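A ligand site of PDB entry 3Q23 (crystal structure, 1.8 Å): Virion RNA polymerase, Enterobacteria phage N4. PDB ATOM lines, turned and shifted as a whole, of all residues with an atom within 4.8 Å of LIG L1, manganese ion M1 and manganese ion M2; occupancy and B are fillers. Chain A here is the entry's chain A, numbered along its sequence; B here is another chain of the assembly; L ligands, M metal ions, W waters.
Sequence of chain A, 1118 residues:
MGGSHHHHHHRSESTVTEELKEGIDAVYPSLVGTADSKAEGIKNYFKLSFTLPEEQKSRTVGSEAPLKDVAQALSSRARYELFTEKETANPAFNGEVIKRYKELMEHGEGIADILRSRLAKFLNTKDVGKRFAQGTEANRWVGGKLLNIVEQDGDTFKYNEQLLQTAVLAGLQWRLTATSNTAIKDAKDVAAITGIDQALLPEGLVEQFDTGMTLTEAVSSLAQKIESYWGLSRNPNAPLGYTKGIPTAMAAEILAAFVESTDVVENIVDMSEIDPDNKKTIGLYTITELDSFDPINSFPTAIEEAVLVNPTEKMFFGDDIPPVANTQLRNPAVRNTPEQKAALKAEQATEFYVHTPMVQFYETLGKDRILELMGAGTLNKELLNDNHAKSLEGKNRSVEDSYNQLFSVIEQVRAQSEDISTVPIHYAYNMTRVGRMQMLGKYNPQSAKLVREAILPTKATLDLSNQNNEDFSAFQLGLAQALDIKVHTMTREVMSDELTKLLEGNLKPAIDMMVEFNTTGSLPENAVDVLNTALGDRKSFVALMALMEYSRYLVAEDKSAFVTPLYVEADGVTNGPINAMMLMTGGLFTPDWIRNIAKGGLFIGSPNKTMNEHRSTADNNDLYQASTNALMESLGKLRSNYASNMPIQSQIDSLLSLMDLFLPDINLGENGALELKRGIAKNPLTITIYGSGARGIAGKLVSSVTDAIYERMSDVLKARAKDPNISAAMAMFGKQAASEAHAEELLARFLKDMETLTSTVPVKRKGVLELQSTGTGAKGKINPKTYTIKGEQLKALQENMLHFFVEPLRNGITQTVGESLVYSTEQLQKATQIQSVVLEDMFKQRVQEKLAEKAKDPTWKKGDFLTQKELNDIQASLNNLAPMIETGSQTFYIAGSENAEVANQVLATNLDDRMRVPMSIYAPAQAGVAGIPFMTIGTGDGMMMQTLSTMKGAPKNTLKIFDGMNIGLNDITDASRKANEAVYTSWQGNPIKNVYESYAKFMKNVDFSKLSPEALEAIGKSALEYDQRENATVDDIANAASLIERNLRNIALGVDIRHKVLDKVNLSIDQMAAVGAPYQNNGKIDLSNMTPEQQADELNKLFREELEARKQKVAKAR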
ATOM      1  N   ARG A 436      31.906  -1.513   0.109  1.00  0.00           N
ATOM      2  CA  ARG A 436      30.713  -2.237  -0.324  1.00  0.00           C
ATOM      3  C   ARG A 436      30.639  -2.310  -1.845  1.00  0.00           C
ATOM      4  O   ARG A 436      31.031  -1.368  -2.532  1.00  0.00           O
ATOM      5  CB  ARG A 436      29.445  -1.597   0.242  1.00  0.00           C
ATOM      6  CG  ARG A 436      29.222  -1.903   1.706  1.00  0.00           C
ATOM      7  CD  ARG A 436      27.977  -1.200   2.190  1.00  0.00           C
ATOM      8  NE  ARG A 436      27.523  -1.729   3.472  1.00  0.00           N
ATOM      9  CZ  ARG A 436      26.434  -1.283   4.098  1.00  0.00           C
ATOM     10  NH1 ARG A 436      25.704  -0.316   3.553  1.00  0.00           N
ATOM     11  NH2 ARG A 436      26.074  -1.805   5.269  1.00  0.00           N
ATOM     12  N   GLU A 569      16.772 -14.955   1.795  1.00  0.00           N
ATOM     13  CA  GLU A 569      17.817 -14.012   2.152  1.00  0.00           C
ATOM     14  C   GLU A 569      18.470 -14.392   3.472  1.00  0.00           C
ATOM     15  O   GLU A 569      17.810 -14.362   4.527  1.00  0.00           O
ATOM     16  CB  GLU A 569      17.270 -12.580   2.258  1.00  0.00           C
ATOM     17  CG  GLU A 569      18.352 -11.538   2.549  1.00  0.00           C
ATOM     18  CD  GLU A 569      17.835 -10.103   2.549  1.00  0.00           C
ATOM     19  OE1 GLU A 569      18.681  -9.192   2.517  1.00  0.00           O
ATOM     20  OE2 GLU A 569      16.604  -9.891   2.585  1.00  0.00           O
ATOM     21  N   ASP A 571      20.550 -12.975   6.180  1.00  0.00           N
ATOM     22  CA  ASP A 571      20.855 -11.602   6.576  1.00  0.00           C
ATOM     23  C   ASP A 571      21.513 -11.530   7.941  1.00  0.00           C
ATOM     24  O   ASP A 571      21.149 -12.272   8.866  1.00  0.00           O
ATOM     25  CB  ASP A 571      19.601 -10.709   6.538  1.00  0.00           C
ATOM     26  CG  ASP A 571      19.913  -9.246   6.803  1.00  0.00           C
ATOM     27  OD1 ASP A 571      20.393  -8.565   5.874  1.00  0.00           O
ATOM     28  OD2 ASP A 571      19.687  -8.767   7.935  1.00  0.00           O
ATOM     29  N   GLY A 572      22.480 -10.618   8.055  1.00  0.00           N
ATOM     30  CA  GLY A 572      23.235 -10.418   9.287  1.00  0.00           C
ATOM     31  C   GLY A 572      22.363  -9.926  10.433  1.00  0.00           C
ATOM     32  O   GLY A 572      21.702  -8.899  10.329  1.00  0.00           O
ATOM     33  N   VAL A 573      22.364 -10.686  11.529  1.00  0.00           N
ATOM     34  CA  VAL A 573      21.584 -10.340  12.705  1.00  0.00           C
ATOM     35  C   VAL A 573      22.267  -9.199  13.445  1.00  0.00           C
ATOM     36  O   VAL A 573      23.389  -9.356  13.925  1.00  0.00           O
ATOM     37  CB  VAL A 573      21.394 -11.557  13.639  1.00  0.00           C
ATOM     38  CG1 VAL A 573      20.606 -11.167  14.889  1.00  0.00           C
ATOM     39  CG2 VAL A 573      20.710 -12.698  12.900  1.00  0.00           C
ATOM     40  N   THR A 574      21.586  -8.056  13.532  1.00  0.00           N
ATOM     41  CA  THR A 574      22.152  -6.844  14.165  1.00  0.00           C
ATOM     42  C   THR A 574      23.620  -6.674  13.753  1.00  0.00           C
ATOM     43  O   THR A 574      24.521  -6.576  14.585  1.00  0.00           O
ATOM     44  CB  THR A 574      21.931  -6.837  15.713  1.00  0.00           C
ATOM     45  OG1 THR A 574      22.714  -7.865  16.321  1.00  0.00           O
ATOM     46  CG2 THR A 574      20.471  -7.101  16.036  1.00  0.00           C
ATOM     47  N   ASN A 575      23.828  -6.639  12.443  1.00  0.00           N
ATOM     48  CA  ASN A 575      25.131  -6.892  11.818  1.00  0.00           C
ATOM     49  C   ASN A 575      26.278  -5.943  12.203  1.00  0.00           C
ATOM     50  O   ASN A 575      27.303  -6.402  12.716  1.00  0.00           O
ATOM     51  CB  ASN A 575      24.929  -6.970  10.285  1.00  0.00           C
ATOM     52  CG  ASN A 575      26.205  -7.282   9.535  1.00  0.00           C
ATOM     53  OD1 ASN A 575      26.595  -8.454   9.395  1.00  0.00           O
ATOM     54  ND2 ASN A 575      26.828  -6.254   9.003  1.00  0.00           N
ATOM     55  N   GLY A 576      26.096  -4.652  11.938  1.00  0.00           N
ATOM     56  CA  GLY A 576      27.113  -3.647  12.246  1.00  0.00           C
ATOM     57  C   GLY A 576      27.534  -3.660  13.707  1.00  0.00           C
ATOM     58  O   GLY A 576      28.729  -3.773  14.014  1.00  0.00           O
ATOM     59  N   PRO A 577      26.561  -3.521  14.633  1.00  0.00           N
ATOM     60  CA  PRO A 577      26.886  -3.600  16.063  1.00  0.00           C
ATOM     61  C   PRO A 577      27.651  -4.865  16.478  1.00  0.00           C
ATOM     62  O   PRO A 577      28.635  -4.776  17.206  1.00  0.00           O
ATOM     63  CB  PRO A 577      25.523  -3.497  16.733  1.00  0.00           C
ATOM     64  CG  PRO A 577      24.714  -2.671  15.758  1.00  0.00           C
ATOM     65  CD  PRO A 577      25.137  -3.227  14.424  1.00  0.00           C
ATOM     66  N   TYR A 624      19.196  -5.409  20.021  1.00  0.00           N
ATOM     67  CA  TYR A 624      18.376  -4.202  20.086  1.00  0.00           C
ATOM     68  C   TYR A 624      17.312  -4.286  21.177  1.00  0.00           C
ATOM     69  O   TYR A 624      17.088  -3.307  21.901  1.00  0.00           O
ATOM     70  CB  TYR A 624      17.774  -3.856  18.722  1.00  0.00           C
ATOM     71  CG  TYR A 624      18.791  -3.669  17.605  1.00  0.00           C
ATOM     72  CD1 TYR A 624      18.490  -4.047  16.288  1.00  0.00           C
ATOM     73  CD2 TYR A 624      20.055  -3.143  17.864  1.00  0.00           C
ATOM     74  CE1 TYR A 624      19.427  -3.899  15.269  1.00  0.00           C
ATOM     75  CE2 TYR A 624      20.997  -2.988  16.840  1.00  0.00           C
ATOM     76  CZ  TYR A 624      20.668  -3.369  15.553  1.00  0.00           C
ATOM     77  OH  TYR A 624      21.592  -3.223  14.537  1.00  0.00           O
ATOM     78  N   ARG A 678      12.130  -3.786  20.168  1.00  0.00           N
ATOM     79  CA  ARG A 678      13.487  -3.602  19.625  1.00  0.00           C
ATOM     80  C   ARG A 678      13.603  -2.438  18.640  1.00  0.00           C
ATOM     81  O   ARG A 678      14.671  -1.839  18.506  1.00  0.00           O
ATOM     82  CB  ARG A 678      13.966  -4.892  18.952  1.00  0.00           C
ATOM     83  CG  ARG A 678      13.269  -5.186  17.621  1.00  0.00           C
ATOM     84  CD  ARG A 678      13.653  -6.535  17.034  1.00  0.00           C
ATOM     85  NE  ARG A 678      15.002  -6.570  16.452  1.00  0.00           N
ATOM     86  CZ  ARG A 678      15.305  -6.163  15.215  1.00  0.00           C
ATOM     87  NH1 ARG A 678      14.381  -5.643  14.419  1.00  0.00           N
ATOM     88  NH2 ARG A 678      16.556  -6.259  14.786  1.00  0.00           N
ATOM     89  N   LYS A 682      16.907   0.101  17.481  1.00  0.00           N
ATOM     90  CA  LYS A 682      17.591  -0.412  16.289  1.00  0.00           C
ATOM     91  C   LYS A 682      18.537   0.613  15.639  1.00  0.00           C
ATOM     92  O   LYS A 682      19.754   0.400  15.607  1.00  0.00           O
ATOM     93  CB  LYS A 682      16.569  -0.939  15.290  1.00  0.00           C
ATOM     94  CG  LYS A 682      17.130  -1.356  13.929  1.00  0.00           C
ATOM     95  CD  LYS A 682      16.164  -2.289  13.213  1.00  0.00           C
ATOM     96  CE  LYS A 682      16.361  -2.293  11.713  1.00  0.00           C
ATOM     97  NZ  LYS A 682      17.786  -2.249  11.335  1.00  0.00           N
ATOM     98  N   ASN A 683      17.990   1.716  15.145  1.00  0.00           N
ATOM     99  CA  ASN A 683      18.813   2.744  14.534  1.00  0.00           C
ATOM    100  C   ASN A 683      19.650   3.543  15.533  1.00  0.00           C
ATOM    101  O   ASN A 683      20.835   3.756  15.292  1.00  0.00           O
ATOM    102  CB  ASN A 683      17.990   3.673  13.634  1.00  0.00           C
ATOM    103  CG  ASN A 683      18.858   4.531  12.736  1.00  0.00           C
ATOM    104  OD1 ASN A 683      19.009   5.737  12.956  1.00  0.00           O
ATOM    105  ND2 ASN A 683      19.464   3.916  11.728  1.00  0.00           N
ATOM    106  N   THR A 686      22.761   1.547  16.490  1.00  0.00           N
ATOM    107  CA  THR A 686      23.627   1.472  15.306  1.00  0.00           C
ATOM    108  C   THR A 686      24.421   2.765  15.107  1.00  0.00           C
ATOM    109  O   THR A 686      25.651   2.739  15.038  1.00  0.00           O
ATOM    110  CB  THR A 686      22.787   1.170  14.043  1.00  0.00           C
ATOM    111  OG1 THR A 686      22.121  -0.084  14.188  1.00  0.00           O
ATOM    112  CG2 THR A 686      23.675   1.123  12.790  1.00  0.00           C
ATOM    113  N   ILE A 687      23.705   3.889  15.057  1.00  0.00           N
ATOM    114  CA  ILE A 687      24.332   5.151  14.691  1.00  0.00           C
ATOM    115  C   ILE A 687      25.118   5.782  15.838  1.00  0.00           C
ATOM    116  O   ILE A 687      26.041   6.571  15.604  1.00  0.00           O
ATOM    117  CB  ILE A 687      23.340   6.126  13.998  1.00  0.00           C
ATOM    118  CG1 ILE A 687      22.336   6.736  14.980  1.00  0.00           C
ATOM    119  CG2 ILE A 687      22.615   5.406  12.847  1.00  0.00           C
ATOM    120  CD1 ILE A 687      21.570   7.925  14.420  1.00  0.00           C
ATOM    121  N   TYR A 690      28.447   4.450  15.541  1.00  0.00           N
ATOM    122  CA  TYR A 690      29.036   5.136  14.389  1.00  0.00           C
ATOM    123  C   TYR A 690      29.295   6.642  14.586  1.00  0.00           C
ATOM    124  O   TYR A 690      29.674   7.336  13.642  1.00  0.00           O
ATOM    125  CB  TYR A 690      28.176   4.909  13.137  1.00  0.00           C
ATOM    126  CG  TYR A 690      28.187   3.475  12.635  1.00  0.00           C
ATOM    127  CD1 TYR A 690      27.125   2.971  11.908  1.00  0.00           C
ATOM    128  CD2 TYR A 690      29.270   2.627  12.903  1.00  0.00           C
ATOM    129  CE1 TYR A 690      27.125   1.659  11.441  1.00  0.00           C
ATOM    130  CE2 TYR A 690      29.280   1.312  12.445  1.00  0.00           C
ATOM    131  CZ  TYR A 690      28.213   0.835  11.710  1.00  0.00           C
ATOM    132  OH  TYR A 690      28.214  -0.458  11.258  1.00  0.00           O
ATOM    133  N   PRO A 933      32.299   4.287  11.099  1.00  0.00           N
ATOM    134  CA  PRO A 933      31.540   3.509  10.096  1.00  0.00           C
ATOM    135  C   PRO A 933      32.379   3.039   8.896  1.00  0.00           C
ATOM    136  O   PRO A 933      32.119   1.946   8.378  1.00  0.00           O
ATOM    137  CB  PRO A 933      30.448   4.475   9.657  1.00  0.00           C
ATOM    138  CG  PRO A 933      30.969   5.837   9.998  1.00  0.00           C
ATOM    139  CD  PRO A 933      31.759   5.644  11.252  1.00  0.00           C
ATOM    140  N   ILE A 937      31.862  -0.903   8.735  1.00  0.00           N
ATOM    141  CA  ILE A 937      31.183  -1.405   7.550  1.00  0.00           C
ATOM    142  C   ILE A 937      32.181  -2.106   6.645  1.00  0.00           C
ATOM    143  O   ILE A 937      31.930  -3.220   6.176  1.00  0.00           O
ATOM    144  CB  ILE A 937      30.417  -0.274   6.803  1.00  0.00           C
ATOM    145  CG1 ILE A 937      29.245   0.220   7.660  1.00  0.00           C
ATOM    146  CG2 ILE A 937      29.927  -0.777   5.444  1.00  0.00           C
ATOM    147  CD1 ILE A 937      28.586   1.525   7.163  1.00  0.00           C
ATOM    148  N   ASP A 941      30.734  -6.096   7.140  1.00  0.00           N
ATOM    149  CA  ASP A 941      29.910  -6.592   6.019  1.00  0.00           C
ATOM    150  C   ASP A 941      30.621  -6.513   4.653  1.00  0.00           C
ATOM    151  O   ASP A 941      30.453  -7.406   3.826  1.00  0.00           O
ATOM    152  CB  ASP A 941      28.491  -5.978   5.988  1.00  0.00           C
ATOM    153  CG  ASP A 941      28.450  -4.497   5.590  1.00  0.00           C
ATOM    154  OD1 ASP A 941      28.845  -4.147   4.450  1.00  0.00           O
ATOM    155  OD2 ASP A 941      27.967  -3.686   6.402  1.00  0.00           O
ATOM    156  N   ILE A 961      23.180  -7.780  -0.951  1.00  0.00           N
ATOM    157  CA  ILE A 961      22.628  -6.497  -0.519  1.00  0.00           C
ATOM    158  C   ILE A 961      23.284  -6.106   0.808  1.00  0.00           C
ATOM    159  O   ILE A 961      22.626  -5.903   1.834  1.00  0.00           O
ATOM    160  CB  ILE A 961      21.078  -6.536  -0.407  1.00  0.00           C
ATOM    161  CG1 ILE A 961      20.467  -7.169  -1.670  1.00  0.00           C
ATOM    162  CG2 ILE A 961      20.511  -5.130  -0.200  1.00  0.00           C
ATOM    163  CD1 ILE A 961      19.064  -7.718  -1.475  1.00  0.00           C
ATOM    164  N   ASP A 963      24.627  -6.598   3.856  1.00  0.00           N
ATOM    165  CA  ASP A 963      24.707  -7.607   4.924  1.00  0.00           C
ATOM    166  C   ASP A 963      23.710  -8.751   4.737  1.00  0.00           C
ATOM    167  O   ASP A 963      23.580  -9.615   5.607  1.00  0.00           O
ATOM    168  CB  ASP A 963      24.523  -6.977   6.296  1.00  0.00           C
ATOM    169  CG  ASP A 963      23.068  -6.839   6.671  1.00  0.00           C
ATOM    170  OD1 ASP A 963      22.289  -6.274   5.858  1.00  0.00           O
ATOM    171  OD2 ASP A 963      22.699  -7.310   7.772  1.00  0.00           O
ATOM    172  N   GLY A 964      22.997  -8.719   3.620  1.00  0.00           N
ATOM    173  CA  GLY A 964      22.065  -9.780   3.246  1.00  0.00           C
ATOM    174  C   GLY A 964      22.393 -10.315   1.872  1.00  0.00           C
ATOM    175  O   GLY A 964      22.888  -9.578   1.017  1.00  0.00           O
ATOM    176  P    DC B  15      25.244  13.969  14.024  1.00  0.00           P
ATOM    177  OP1  DC B  15      23.941  13.953  13.321  1.00  0.00           O
ATOM    178  OP2  DC B  15      26.210  15.053  13.719  1.00  0.00           O
ATOM    179  O5'  DC B  15      25.989  12.599  13.698  1.00  0.00           O
ATOM    180  C5'  DC B  15      26.376  12.335  12.355  1.00  0.00           C
ATOM    181  C4'  DC B  15      27.163  11.033  12.321  1.00  0.00           C
ATOM    182  O4'  DC B  15      26.366   9.988  12.911  1.00  0.00           O
ATOM    183  C3'  DC B  15      27.468  10.551  10.912  1.00  0.00           C
ATOM    184  O3'  DC B  15      28.656  11.167  10.439  1.00  0.00           O
ATOM    185  C2'  DC B  15      27.646   9.049  11.156  1.00  0.00           C
ATOM    186  C1'  DC B  15      26.490   8.802  12.141  1.00  0.00           C
ATOM    187  N1   DC B  15      25.175   8.482  11.485  1.00  0.00           N
ATOM    188  C2   DC B  15      25.025   7.229  10.868  1.00  0.00           C
ATOM    189  O2   DC B  15      25.971   6.421  10.893  1.00  0.00           O
ATOM    190  N3   DC B  15      23.834   6.946  10.278  1.00  0.00           N
ATOM    191  C4   DC B  15      22.833   7.830  10.271  1.00  0.00           C
ATOM    192  N4   DC B  15      21.684   7.485   9.671  1.00  0.00           N
ATOM    193  C5   DC B  15      22.975   9.106  10.892  1.00  0.00           C
ATOM    194  C6   DC B  15      24.149   9.384  11.477  1.00  0.00           C
ATOM    195  P    DC B  16      28.755  11.623   8.907  1.00  0.00           P
ATOM    196  OP1  DC B  16      30.035  12.345   8.766  1.00  0.00           O
ATOM    197  OP2  DC B  16      27.498  12.243   8.477  1.00  0.00           O
ATOM    198  O5'  DC B  16      28.874  10.225   8.138  1.00  0.00           O
ATOM    199  C5'  DC B  16      30.103   9.520   8.191  1.00  0.00           C
ATOM    200  C4'  DC B  16      30.002   8.227   7.415  1.00  0.00           C
ATOM    201  O4'  DC B  16      28.978   7.416   8.028  1.00  0.00           O
ATOM    202  C3'  DC B  16      29.530   8.359   5.978  1.00  0.00           C
ATOM    203  O3'  DC B  16      30.624   8.748   5.151  1.00  0.00           O
ATOM    204  C2'  DC B  16      29.073   6.935   5.711  1.00  0.00           C
ATOM    205  C1'  DC B  16      28.413   6.584   7.042  1.00  0.00           C
ATOM    206  N1   DC B  16      26.923   6.742   6.995  1.00  0.00           N
ATOM    207  C2   DC B  16      26.150   5.674   6.500  1.00  0.00           C
ATOM    208  O2   DC B  16      26.709   4.642   6.119  1.00  0.00           O
ATOM    209  N3   DC B  16      24.802   5.807   6.450  1.00  0.00           N
ATOM    210  C4   DC B  16      24.213   6.935   6.869  1.00  0.00           C
ATOM    211  N4   DC B  16      22.878   6.999   6.786  1.00  0.00           N
ATOM    212  C5   DC B  16      24.975   8.038   7.365  1.00  0.00           C
ATOM    213  C6   DC B  16      26.307   7.901   7.409  1.00  0.00           C
HETATM  214  P1  LIG L   1      18.710  -6.807  11.744  1.00  0.00           P
HETATM  215  O1  LIG L   1      19.013  -7.174  10.294  1.00  0.00           O
HETATM  216  O2  LIG L   1      17.384  -6.108  11.878  1.00  0.00           O
HETATM  217  O3  LIG L   1      18.918  -7.933  12.716  1.00  0.00           O
HETATM  218  O4  LIG L   1      19.800  -5.695  12.204  1.00  0.00           O
HETATM  219  P2  LIG L   1      20.739  -4.862  11.179  1.00  0.00           P
HETATM  220  O5  LIG L   1      21.618  -5.874  10.466  1.00  0.00           O
HETATM  221  O6  LIG L   1      21.444  -3.775  11.976  1.00  0.00           O
HETATM  222  C1  LIG L   1      19.590  -4.034  10.042  1.00  0.00           C
HETATM  223  P3  LIG L   1      20.061  -4.078   8.286  1.00  0.00           P
HETATM  224  O7  LIG L   1      19.038  -3.285   7.513  1.00  0.00           O
HETATM  225  O8  LIG L   1      20.253  -5.517   7.874  1.00  0.00           O
HETATM  226  O9  LIG L   1      21.447  -3.262   8.164  1.00  0.00           O
HETATM  227  C2  LIG L   1      22.703  -3.914   8.148  1.00  0.00           C
HETATM  228  C3  LIG L   1      23.815  -2.931   8.497  1.00  0.00           C
HETATM  229  O10 LIG L   1      23.807  -1.796   7.616  1.00  0.00           O
HETATM  230  C4  LIG L   1      23.656  -2.315   9.879  1.00  0.00           C
HETATM  231  O11 LIG L   1      23.959  -3.204  10.973  1.00  0.00           O
HETATM  232  C5  LIG L   1      24.576  -1.118   9.750  1.00  0.00           C
HETATM  233  O12 LIG L   1      25.951  -1.466   9.914  1.00  0.00           O
HETATM  234  C6  LIG L   1      24.297  -0.652   8.323  1.00  0.00           C
HETATM  235  N1  LIG L   1      23.269   0.406   8.478  1.00  0.00           N
HETATM  236  C7  LIG L   1      21.927   0.276   8.477  1.00  0.00           C
HETATM  237  N2  LIG L   1      21.368   1.490   8.717  1.00  0.00           N
HETATM  238  C8  LIG L   1      22.375   2.375   8.886  1.00  0.00           C
HETATM  239  C9  LIG L   1      22.441   3.738   9.157  1.00  0.00           C
HETATM  240  O13 LIG L   1      21.405   4.426   9.293  1.00  0.00           O
HETATM  241  N3  LIG L   1      23.656   4.328   9.263  1.00  0.00           N
HETATM  242  C10 LIG L   1      24.805   3.624   9.128  1.00  0.00           C
HETATM  243  N4  LIG L   1      26.006   4.229   9.243  1.00  0.00           N
HETATM  244  N5  LIG L   1      24.767   2.301   8.869  1.00  0.00           N
HETATM  245  C11 LIG L   1      23.572   1.670   8.740  1.00  0.00           C
HETATM  246  P1  LG2 L   2      17.208  -6.359   4.599  1.00  0.00           P
HETATM  247  O1  LG2 L   2      17.824  -6.734   3.264  1.00  0.00           O
HETATM  248  O2  LG2 L   2      15.987  -7.162   4.950  1.00  0.00           O
HETATM  249  O3  LG2 L   2      18.219  -6.219   5.716  1.00  0.00           O
HETATM  250  O4  LG2 L   2      16.747  -4.841   4.296  1.00  0.00           O
HETATM  251  P2  LG2 L   2      15.463  -4.053   4.888  1.00  0.00           P
HETATM  252  O5  LG2 L   2      15.305  -4.439   6.344  1.00  0.00           O
HETATM  253  O6  LG2 L   2      14.291  -4.289   3.951  1.00  0.00           O
HETATM  254  C1  LG2 L   2      15.878  -2.289   4.794  1.00  0.00           C
HETATM  255  P3  LG2 L   2      16.511  -1.748   3.173  1.00  0.00           P
HETATM  256  O7  LG2 L   2      16.033  -2.702   2.102  1.00  0.00           O
HETATM  257  O8  LG2 L   2      16.147  -0.294   3.065  1.00  0.00           O
HETATM  258  O9  LG2 L   2      18.116  -1.748   3.192  1.00  0.00           O
HETATM  259  C2  LG2 L   2      18.909  -2.709   2.481  1.00  0.00           C
HETATM  260  C3  LG2 L   2      20.306  -2.753   3.075  1.00  0.00           C
HETATM  261  O10 LG2 L   2      21.068  -1.576   2.762  1.00  0.00           O
HETATM  262  C4  LG2 L   2      20.291  -2.804   4.596  1.00  0.00           C
HETATM  263  O11 LG2 L   2      20.046  -4.111   5.129  1.00  0.00           O
HETATM  264  C5  LG2 L   2      21.662  -2.263   4.955  1.00  0.00           C
HETATM  265  O12 LG2 L   2      22.643  -3.302   4.793  1.00  0.00           O
HETATM  266  C6  LG2 L   2      21.880  -1.200   3.896  1.00  0.00           C
HETATM  267  N1  LG2 L   2      21.468   0.142   4.404  1.00  0.00           N
HETATM  268  C7  LG2 L   2      20.213   0.614   4.516  1.00  0.00           C
HETATM  269  N2  LG2 L   2      20.250   1.876   5.015  1.00  0.00           N
HETATM  270  C8  LG2 L   2      21.538   2.195   5.222  1.00  0.00           C
HETATM  271  C9  LG2 L   2      22.166   3.335   5.703  1.00  0.00           C
HETATM  272  O13 LG2 L   2      21.499   4.337   6.054  1.00  0.00           O
HETATM  273  N3  LG2 L   2      23.527   3.358   5.781  1.00  0.00           N
HETATM  274  C10 LG2 L   2      24.263   2.280   5.408  1.00  0.00           C
HETATM  275  N4  LG2 L   2      25.601   2.307   5.490  1.00  0.00           N
HETATM  276  N5  LG2 L   2      23.650   1.161   4.938  1.00  0.00           N
HETATM  277  C11 LG2 L   2      22.299   1.101   4.827  1.00  0.00           C
HETATM  278 MN    MN M   1      20.276  -6.431   5.738  1.00  0.00          MN
HETATM  279 MN    MN M   2      20.892  -7.334   9.112  1.00  0.00          MN
HETATM  280  O   HOH W   1      16.565  -3.343   8.368  1.00  0.00           O
HETATM  281  O   HOH W   2      18.611   2.014   8.181  1.00  0.00           O
HETATM  282  O   HOH W   3      17.568 -10.122  12.667  1.00  0.00           O
HETATM  283  O   HOH W   4      20.405  -6.527   3.353  1.00  0.00           O
HETATM  284  O   HOH W   5      27.083  -3.674   8.873  1.00  0.00           O
HETATM  285  O   HOH W   6      14.237  -6.420  10.720  1.00  0.00           O
HETATM  286  O   HOH W   7      18.482 -10.554  10.132  1.00  0.00           O
HETATM  287  O   HOH W   8      21.073  -1.017  11.873  1.00  0.00           O
HETATM  288  O   HOH W   9      18.866  -0.592   7.485  1.00  0.00           O
HETATM  289  O   HOH W  10      17.109  -6.959   8.290  1.00  0.00           O
HETATM  290  O   HOH W  11      19.099   5.302   8.364  1.00  0.00           O
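ND2 of Asn 683 sits at hydrogen-bond distance from O13 of LIG L1.
The guanidinium group (NH1) of Arg 436 lies within hydrogen-bond range of a nitrogen (N5) of LG2 L2 (2.9 Å).
OH of Tyr 624 sits at hydrogen-bond distance from O6 of LIG L1, 2.6 Å away.
N of Thr 574 is in hydrogen-bond range of O3 of LIG L1, 2.8 Å away.
O2 of DC 16 of chain B lies close to a nitrogen (N4) of LIG L1 (3.2 Å).
The side-chain carboxylate of Glu 569 lies close to an oxygen (O1) of LG2 L2 (2.7 Å).
NH2 of Arg 436 lies within hydrogen-bond range of O10 of LIG L1 (3.3 Å).
The backbone NH of Asn 575 lies close to an oxygen (O5) of LIG L1 (3.1 Å).
The backbone NH (N) of Gly 576 lies within hydrogen-bond range of an oxygen (O11) of LIG L1 (2.8 Å).
OH of Tyr 690 lies within hydrogen-bond range of O12 of LIG L1 (2.8 Å).
The guanidinium group (NH2) of Arg 678 is in salt-bridge range of an oxygen (O2) of LIG L1 (3.0 Å).
O2 of DC 15 of chain B is in hydrogen-bond range of N4 of LIG L1, 2.7 Å away.
O2 of DC 16 of chain B sits at hydrogen-bond distance from N4 of LG2 L2, at 2.7 Å.
NZ of Lys 682 lies within salt-bridge range of O2 of LIG L1, 3.9 Å away.
The side-chain carboxylate (OD1) of Asp 571 lies close to the backbone NH (N) of Gly 964 (3.4 Å).
The side-chain carboxylate of Asp 941 lies within salt-bridge range of the guanidinium group of Arg 436 (2.9 Å).
OH of Tyr 624 sits at hydrogen-bond distance from OG1 of Thr 686 (3.2 Å).
The side-chain hydroxyl (OG1) of Thr 686 is in hydrogen-bond range of the backbone carbonyl oxygen (O) of Lys 682 (2.8 Å).
Val 573 touches LIG L1.
CD of Pro 577 touches O11 of LIG L1, at 3.6 Å.
CG2 of Thr 686 touches C5 of LIG L1, 3.9 Å away.
CG2 of Ile 687 touches O13 of LIG L1, at 3.9 Å.
Hydrophobic or aromatic side chains that line LIG L1: Pro 577, Tyr 624, Ile 687 and Tyr 690.
Within 4 Å of LIG L1: Arg 436, Asp 571, Gly 572, Val 573, Thr 574, Asn 575, Gly 576, Pro 577, Tyr 624, Arg 678, Lys 682, Asn 683, Thr 686, Ile 687, Tyr 690, Asp 963, DC 15 of chain B and DC 16 of chain B.
The nearest printed residue that does not touch LIG L1 is Ile 937 (4.3 Å).
Of the 24 residues printed, 2 come within 4 Å of manganese ion M1.
Of the 24 residues printed, 3 come within 4 Å of manganese ion M2.
The nearest printed residue that does not touch manganese ion M2 is Asn 575 (4.2 Å).
Manganese ion M1 is bound by the side-chain carboxylate (OD1) of Asp 963 (2.0 Å), an oxygen (O3) of LG2 L2 (2.1 Å), the side-chain carboxylate (OD1) of Asp 571 (2.1 Å), an oxygen (O8) of LIG L1 (2.3 Å), water W4 (2.4 Å) and an oxygen (O11) of LG2 L2 (2.4 Å).
Manganese ion M1 has six donor atoms within binding distance.
Manganese ion M2 is bound by O5 of LIG L1 (2.1 Å), O of Gly 572 (2.1 Å), OD2 of Asp 571 (2.2 Å), O1 of LIG L1 (2.2 Å), OD2 of Asp 963 (2.2 Å) and O8 of LIG L1 (2.3 Å).
Water W4 lies within hydrogen-bond range of O1 of LG2 L2, O of Ile 961, OE1 of Glu 569 and N of Gly 964.
Water W1 lies within hydrogen-bond range of O7 of LIG L1, O5 of LG2 L2 and NZ of Lys 682.
Water W11 bridges O13 of LIG L1 (2.6 Å) and O13 of LG2 L2 (3.5 Å).
Water W5 lies within hydrogen-bond range of ND2 of Asn 575 (2.6 Å), OD2 of Asp 941 (2.6 Å), O12 of LIG L1 (2.7 Å) and N of Gly 576 (3.4 Å).
Water W8 lies within hydrogen-bond range of OG1 of Thr 686 (2.7 Å), O6 of LIG L1 (2.8 Å) and OH of Tyr 624 (3.5 Å).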
